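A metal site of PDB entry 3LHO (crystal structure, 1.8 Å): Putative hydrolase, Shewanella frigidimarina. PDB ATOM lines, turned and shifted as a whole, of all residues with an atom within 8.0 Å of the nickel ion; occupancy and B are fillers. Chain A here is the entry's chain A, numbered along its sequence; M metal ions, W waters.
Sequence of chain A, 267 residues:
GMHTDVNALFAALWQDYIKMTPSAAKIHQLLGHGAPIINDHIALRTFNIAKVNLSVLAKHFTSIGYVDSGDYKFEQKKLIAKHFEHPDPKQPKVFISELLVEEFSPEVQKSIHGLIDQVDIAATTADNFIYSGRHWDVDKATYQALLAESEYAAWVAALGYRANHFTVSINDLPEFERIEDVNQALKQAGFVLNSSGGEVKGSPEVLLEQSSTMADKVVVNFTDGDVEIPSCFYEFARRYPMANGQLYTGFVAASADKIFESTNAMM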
ATOM      1  N   ASP A  40     -29.572 -10.409 -15.667  1.00  0.00           N
ATOM      2  CA  ASP A  40     -29.900  -9.044 -16.088  1.00  0.00           C
ATOM      3  C   ASP A  40     -28.682  -8.331 -16.673  1.00  0.00           C
ATOM      4  O   ASP A  40     -28.758  -7.651 -17.710  1.00  0.00           O
ATOM      5  CB  ASP A  40     -30.376  -8.214 -14.869  1.00  0.00           C
ATOM      6  CG  ASP A  40     -30.766  -6.801 -15.256  1.00  0.00           C
ATOM      7  OD1 ASP A  40     -31.763  -6.665 -15.974  1.00  0.00           O
ATOM      8  OD2 ASP A  40     -30.052  -5.814 -14.950  1.00  0.00           O
ATOM      9  N   HIS A  41     -27.543  -8.482 -15.980  1.00  0.00           N
ATOM     10  CA  HIS A  41     -26.298  -7.835 -16.380  1.00  0.00           C
ATOM     11  C   HIS A  41     -25.088  -8.417 -15.719  1.00  0.00           C
ATOM     12  O   HIS A  41     -25.217  -9.201 -14.753  1.00  0.00           O
ATOM     13  CB  HIS A  41     -26.351  -6.281 -16.170  1.00  0.00           C
ATOM     14  CG  HIS A  41     -26.384  -5.815 -14.742  1.00  0.00           C
ATOM     15  ND1 HIS A  41     -27.565  -5.591 -14.052  1.00  0.00           N
ATOM     16  CD2 HIS A  41     -25.380  -5.397 -13.916  1.00  0.00           C
ATOM     17  CE1 HIS A  41     -27.289  -5.118 -12.854  1.00  0.00           C
ATOM     18  NE2 HIS A  41     -25.983  -4.967 -12.753  1.00  0.00           N
ATOM     19  N   ILE A  42     -23.928  -8.087 -16.320  1.00  0.00           N
ATOM     20  CA  ILE A  42     -22.613  -8.125 -15.679  1.00  0.00           C
ATOM     21  C   ILE A  42     -22.049  -6.696 -15.608  1.00  0.00           C
ATOM     22  O   ILE A  42     -22.527  -5.750 -16.303  1.00  0.00           O
ATOM     23  CB  ILE A  42     -21.617  -9.139 -16.382  1.00  0.00           C
ATOM     24  CG1 ILE A  42     -21.319  -8.708 -17.827  1.00  0.00           C
ATOM     25  CG2 ILE A  42     -22.183 -10.571 -16.370  1.00  0.00           C
ATOM     26  CD1 ILE A  42     -19.927  -8.526 -18.162  1.00  0.00           C
ATOM     27  N   ALA A  43     -21.100  -6.511 -14.691  1.00  0.00           N
ATOM     28  CA  ALA A  43     -20.457  -5.200 -14.511  1.00  0.00           C
ATOM     29  C   ALA A  43     -18.951  -5.391 -14.558  1.00  0.00           C
ATOM     30  O   ALA A  43     -18.426  -6.285 -13.858  1.00  0.00           O
ATOM     31  CB  ALA A  43     -20.844  -4.587 -13.159  1.00  0.00           C
ATOM     32  N   PHE A  95     -22.527  -3.764 -18.488  1.00  0.00           N
ATOM     33  CA  PHE A  95     -22.296  -2.476 -17.922  1.00  0.00           C
ATOM     34  C   PHE A  95     -20.777  -2.325 -17.714  1.00  0.00           C
ATOM     35  O   PHE A  95     -20.159  -3.174 -17.014  1.00  0.00           O
ATOM     36  CB  PHE A  95     -23.004  -2.391 -16.597  1.00  0.00           C
ATOM     37  CG  PHE A  95     -22.945  -1.035 -15.967  1.00  0.00           C
ATOM     38  CD1 PHE A  95     -23.817  -0.024 -16.362  1.00  0.00           C
ATOM     39  CD2 PHE A  95     -21.989  -0.775 -14.965  1.00  0.00           C
ATOM     40  CE1 PHE A  95     -23.750   1.267 -15.780  1.00  0.00           C
ATOM     41  CE2 PHE A  95     -21.913   0.468 -14.363  1.00  0.00           C
ATOM     42  CZ  PHE A  95     -22.801   1.521 -14.773  1.00  0.00           C
ATOM     43  N   ASN A 164     -16.887  -7.779 -11.856  1.00  0.00           N
ATOM     44  CA  ASN A 164     -17.171  -7.250 -10.538  1.00  0.00           C
ATOM     45  C   ASN A 164     -18.421  -7.895  -9.961  1.00  0.00           C
ATOM     46  O   ASN A 164     -18.452  -8.202  -8.774  1.00  0.00           O
ATOM     47  CB  ASN A 164     -17.347  -5.733 -10.569  1.00  0.00           C
ATOM     48  CG  ASN A 164     -17.735  -5.144  -9.180  1.00  0.00           C
ATOM     49  OD1 ASN A 164     -18.898  -4.898  -8.909  1.00  0.00           O
ATOM     50  ND2 ASN A 164     -16.749  -4.925  -8.298  1.00  0.00           N
ATOM     51  N   HIS A 165     -19.432  -8.097 -10.794  1.00  0.00           N
ATOM     52  CA  HIS A 165     -20.606  -8.919 -10.392  1.00  0.00           C
ATOM     53  C   HIS A 165     -21.416  -9.396 -11.576  1.00  0.00           C
ATOM     54  O   HIS A 165     -21.347  -8.816 -12.670  1.00  0.00           O
ATOM     55  CB  HIS A 165     -21.513  -8.179  -9.378  1.00  0.00           C
ATOM     56  CG  HIS A 165     -22.103  -6.895  -9.861  1.00  0.00           C
ATOM     57  ND1 HIS A 165     -21.481  -5.677  -9.699  1.00  0.00           N
ATOM     58  CD2 HIS A 165     -23.316  -6.620 -10.400  1.00  0.00           C
ATOM     59  CE1 HIS A 165     -22.252  -4.713 -10.174  1.00  0.00           C
ATOM     60  NE2 HIS A 165     -23.366  -5.268 -10.625  1.00  0.00           N
ATOM     61  N   PHE A 166     -22.124 -10.508 -11.355  1.00  0.00           N
ATOM     62  CA  PHE A 166     -23.291 -10.900 -12.155  1.00  0.00           C
ATOM     63  C   PHE A 166     -24.548 -10.535 -11.404  1.00  0.00           C
ATOM     64  O   PHE A 166     -24.567 -10.571 -10.168  1.00  0.00           O
ATOM     65  CB  PHE A 166     -23.288 -12.380 -12.350  1.00  0.00           C
ATOM     66  CG  PHE A 166     -22.353 -12.826 -13.395  1.00  0.00           C
ATOM     67  CD1 PHE A 166     -20.986 -12.728 -13.199  1.00  0.00           C
ATOM     68  CD2 PHE A 166     -22.849 -13.376 -14.586  1.00  0.00           C
ATOM     69  CE1 PHE A 166     -20.108 -13.166 -14.188  1.00  0.00           C
ATOM     70  CE2 PHE A 166     -21.953 -13.843 -15.561  1.00  0.00           C
ATOM     71  CZ  PHE A 166     -20.606 -13.680 -15.380  1.00  0.00           C
ATOM     72  N   THR A 167     -25.606 -10.217 -12.165  1.00  0.00           N
ATOM     73  CA  THR A 167     -26.902  -9.895 -11.621  1.00  0.00           C
ATOM     74  C   THR A 167     -28.014 -10.738 -12.233  1.00  0.00           C
ATOM     75  O   THR A 167     -28.212 -10.706 -13.456  1.00  0.00           O
ATOM     76  CB  THR A 167     -27.240  -8.417 -11.844  1.00  0.00           C
ATOM     77  OG1 THR A 167     -26.217  -7.601 -11.247  1.00  0.00           O
ATOM     78  CG2 THR A 167     -28.632  -8.108 -11.218  1.00  0.00           C
ATOM     79  N   LEU A 208     -36.929   0.063 -10.986  1.00  0.00           N
ATOM     80  CA  LEU A 208     -35.791  -0.813 -10.768  1.00  0.00           C
ATOM     81  C   LEU A 208     -35.659  -1.138  -9.281  1.00  0.00           C
ATOM     82  O   LEU A 208     -35.678  -0.248  -8.442  1.00  0.00           O
ATOM     83  CB  LEU A 208     -34.488  -0.175 -11.295  1.00  0.00           C
ATOM     84  CG  LEU A 208     -33.187  -0.974 -11.084  1.00  0.00           C
ATOM     85  CD1 LEU A 208     -33.280  -2.276 -11.836  1.00  0.00           C
ATOM     86  CD2 LEU A 208     -31.929  -0.186 -11.557  1.00  0.00           C
ATOM     87  N   GLN A 210     -33.100  -3.583  -6.709  1.00  0.00           N
ATOM     88  CA  GLN A 210     -31.914  -4.428  -6.649  1.00  0.00           C
ATOM     89  C   GLN A 210     -31.611  -4.836  -5.224  1.00  0.00           C
ATOM     90  O   GLN A 210     -31.966  -4.123  -4.281  1.00  0.00           O
ATOM     91  CB  GLN A 210     -30.687  -3.722  -7.274  1.00  0.00           C
ATOM     92  CG  GLN A 210     -30.802  -3.456  -8.767  1.00  0.00           C
ATOM     93  CD  GLN A 210     -29.558  -2.784  -9.365  1.00  0.00           C
ATOM     94  OE1 GLN A 210     -29.286  -1.629  -9.108  1.00  0.00           O
ATOM     95  NE2 GLN A 210     -28.812  -3.532 -10.166  1.00  0.00           N
ATOM     96  N   SER A 211     -30.992  -5.996  -5.079  1.00  0.00           N
ATOM     97  CA  SER A 211     -30.517  -6.483  -3.800  1.00  0.00           C
ATOM     98  C   SER A 211     -29.244  -7.263  -4.086  1.00  0.00           C
ATOM     99  O   SER A 211     -28.948  -7.529  -5.250  1.00  0.00           O
ATOM    100  CB  SER A 211     -31.582  -7.383  -3.169  1.00  0.00           C
ATOM    101  OG  SER A 211     -31.718  -8.566  -3.925  1.00  0.00           O
ATOM    102  N   PHE A 233     -19.900  -9.349  -4.514  1.00  0.00           N
ATOM    103  CA  PHE A 233     -21.242  -9.802  -4.265  1.00  0.00           C
ATOM    104  C   PHE A 233     -21.906 -10.363  -5.554  1.00  0.00           C
ATOM    105  O   PHE A 233     -21.385 -10.183  -6.653  1.00  0.00           O
ATOM    106  CB  PHE A 233     -22.112  -8.671  -3.689  1.00  0.00           C
ATOM    107  CG  PHE A 233     -22.126  -7.416  -4.501  1.00  0.00           C
ATOM    108  CD1 PHE A 233     -22.854  -7.352  -5.701  1.00  0.00           C
ATOM    109  CD2 PHE A 233     -21.450  -6.280  -4.086  1.00  0.00           C
ATOM    110  CE1 PHE A 233     -22.866  -6.193  -6.475  1.00  0.00           C
ATOM    111  CE2 PHE A 233     -21.475  -5.115  -4.829  1.00  0.00           C
ATOM    112  CZ  PHE A 233     -22.199  -5.068  -6.043  1.00  0.00           C
ATOM    113  N   GLU A 235     -25.747 -10.106  -7.267  1.00  0.00           N
ATOM    114  CA  GLU A 235     -26.820  -9.119  -7.284  1.00  0.00           C
ATOM    115  C   GLU A 235     -28.086  -9.688  -7.947  1.00  0.00           C
ATOM    116  O   GLU A 235     -28.026 -10.676  -8.666  1.00  0.00           O
ATOM    117  CB  GLU A 235     -26.325  -7.911  -8.035  1.00  0.00           C
ATOM    118  CG  GLU A 235     -27.158  -6.628  -7.908  1.00  0.00           C
ATOM    119  CD  GLU A 235     -26.441  -5.420  -8.534  1.00  0.00           C
ATOM    120  OE1 GLU A 235     -26.441  -5.319  -9.785  1.00  0.00           O
ATOM    121  OE2 GLU A 235     -25.862  -4.581  -7.792  1.00  0.00           O
ATOM    122  N   PHE A 236     -29.223  -9.041  -7.665  1.00  0.00           N
ATOM    123  CA  PHE A 236     -30.574  -9.443  -8.135  1.00  0.00           C
ATOM    124  C   PHE A 236     -31.284  -8.192  -8.556  1.00  0.00           C
ATOM    125  O   PHE A 236     -31.236  -7.201  -7.866  1.00  0.00           O
ATOM    126  CB  PHE A 236     -31.320 -10.194  -7.013  1.00  0.00           C
ATOM    127  CG  PHE A 236     -30.473 -11.278  -6.390  1.00  0.00           C
ATOM    128  CD1 PHE A 236     -30.461 -12.551  -6.915  1.00  0.00           C
ATOM    129  CD2 PHE A 236     -29.613 -10.998  -5.332  1.00  0.00           C
ATOM    130  CE1 PHE A 236     -29.609 -13.519  -6.383  1.00  0.00           C
ATOM    131  CE2 PHE A 236     -28.767 -11.980  -4.807  1.00  0.00           C
ATOM    132  CZ  PHE A 236     -28.762 -13.217  -5.342  1.00  0.00           C
ATOM    133  N   ALA A 237     -31.912  -8.196  -9.731  1.00  0.00           N
ATOM    134  CA  ALA A 237     -32.589  -7.002 -10.216  1.00  0.00           C
ATOM    135  C   ALA A 237     -33.957  -7.353 -10.806  1.00  0.00           C
ATOM    136  O   ALA A 237     -34.085  -8.302 -11.590  1.00  0.00           O
ATOM    137  CB  ALA A 237     -31.721  -6.276 -11.292  1.00  0.00           C
ATOM    138  N   ARG A 239     -36.677  -5.315 -13.134  1.00  0.00           N
ATOM    139  CA  ARG A 239     -37.025  -4.131 -13.907  1.00  0.00           C
ATOM    140  C   ARG A 239     -38.500  -4.022 -14.236  1.00  0.00           C
ATOM    141  O   ARG A 239     -39.180  -5.045 -14.397  1.00  0.00           O
ATOM    142  CB  ARG A 239     -36.235  -4.101 -15.205  1.00  0.00           C
ATOM    143  CG  ARG A 239     -34.746  -4.013 -15.011  1.00  0.00           C
ATOM    144  CD  ARG A 239     -34.022  -4.176 -16.364  1.00  0.00           C
ATOM    145  NE  ARG A 239     -32.606  -4.096 -16.092  1.00  0.00           N
ATOM    146  CZ  ARG A 239     -31.952  -2.979 -15.780  1.00  0.00           C
ATOM    147  NH1 ARG A 239     -32.570  -1.784 -15.765  1.00  0.00           N
ATOM    148  NH2 ARG A 239     -30.687  -3.053 -15.469  1.00  0.00           N
ATOM    149  N   PHE A 251     -29.360   1.802 -14.604  1.00  0.00           N
ATOM    150  CA  PHE A 251     -28.626   1.045 -13.582  1.00  0.00           C
ATOM    151  C   PHE A 251     -28.642   1.636 -12.170  1.00  0.00           C
ATOM    152  O   PHE A 251     -28.111   1.019 -11.220  1.00  0.00           O
ATOM    153  CB  PHE A 251     -27.197   0.754 -14.079  1.00  0.00           C
ATOM    154  CG  PHE A 251     -27.168  -0.276 -15.150  1.00  0.00           C
ATOM    155  CD1 PHE A 251     -27.376   0.083 -16.465  1.00  0.00           C
ATOM    156  CD2 PHE A 251     -27.050  -1.617 -14.826  1.00  0.00           C
ATOM    157  CE1 PHE A 251     -27.415  -0.853 -17.431  1.00  0.00           C
ATOM    158  CE2 PHE A 251     -27.084  -2.570 -15.806  1.00  0.00           C
ATOM    159  CZ  PHE A 251     -27.273  -2.190 -17.110  1.00  0.00           C
HETATM  160 NI    NI M   1     -25.116  -4.112 -10.995  1.00  0.00          NI
HETATM  161  O   HOH W   1     -26.487  -2.610 -11.071  1.00  0.00           O
HETATM  162  O   HOH W   2     -24.738  -2.617  -9.141  1.00  0.00           O
HETATM  163  O   HOH W   3     -24.174  -2.306 -12.041  1.00  0.00           O
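The nickel ion is bound by water W1 (2.0 Å), NE2 of His 165 (2.1 Å), NE2 of His 41 (2.1 Å), OE1 of Glu 235 (2.2 Å), water W3 (2.3 Å) and water W2 (2.4 Å).
The nickel ion has six donor atoms within binding distance.
Thr 167 touches the nickel ion.
NE2 of Gln 210 touches the nickel ion, at 3.8 Å.
Of the 18 residues printed, 5 come within 4 Å of the nickel ion.
Along chain A the residues within 4 Å of the nickel ion span positions 41 to 235.
The backbone NH (N) of Ala 43 sits at hydrogen-bond distance from the backbone carbonyl oxygen (O) of His 165 (3.1 Å).
ND1 of His 165 is in hydrogen-bond range of OD1 of Asn 164, at 2.8 Å.
O of His 41 sits at hydrogen-bond distance from N of Thr 167, 2.8 Å away.
ND1 of His 41 sits at hydrogen-bond distance from OD2 of Asp 40 (2.7 Å).
The side-chain hydroxyl (OG1) of Thr 167 sits close to the side-chain carboxylate (OE1) of Glu 235, 2.7 Å away.
The side-chain carboxylate (OE1) of Glu 235 lies close to the side-chain amide nitrogen (NE2) of Gln 210, 3.0 Å away.
The backbone carbonyl oxygen (O) of Phe 166 is in hydrogen-bond range of the backbone NH (N) of Glu 235 (3.2 Å).
The backbone carbonyl oxygen (O) of Thr 167 sits at hydrogen-bond distance from the backbone NH (N) of Asp 40, at 2.6 Å.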
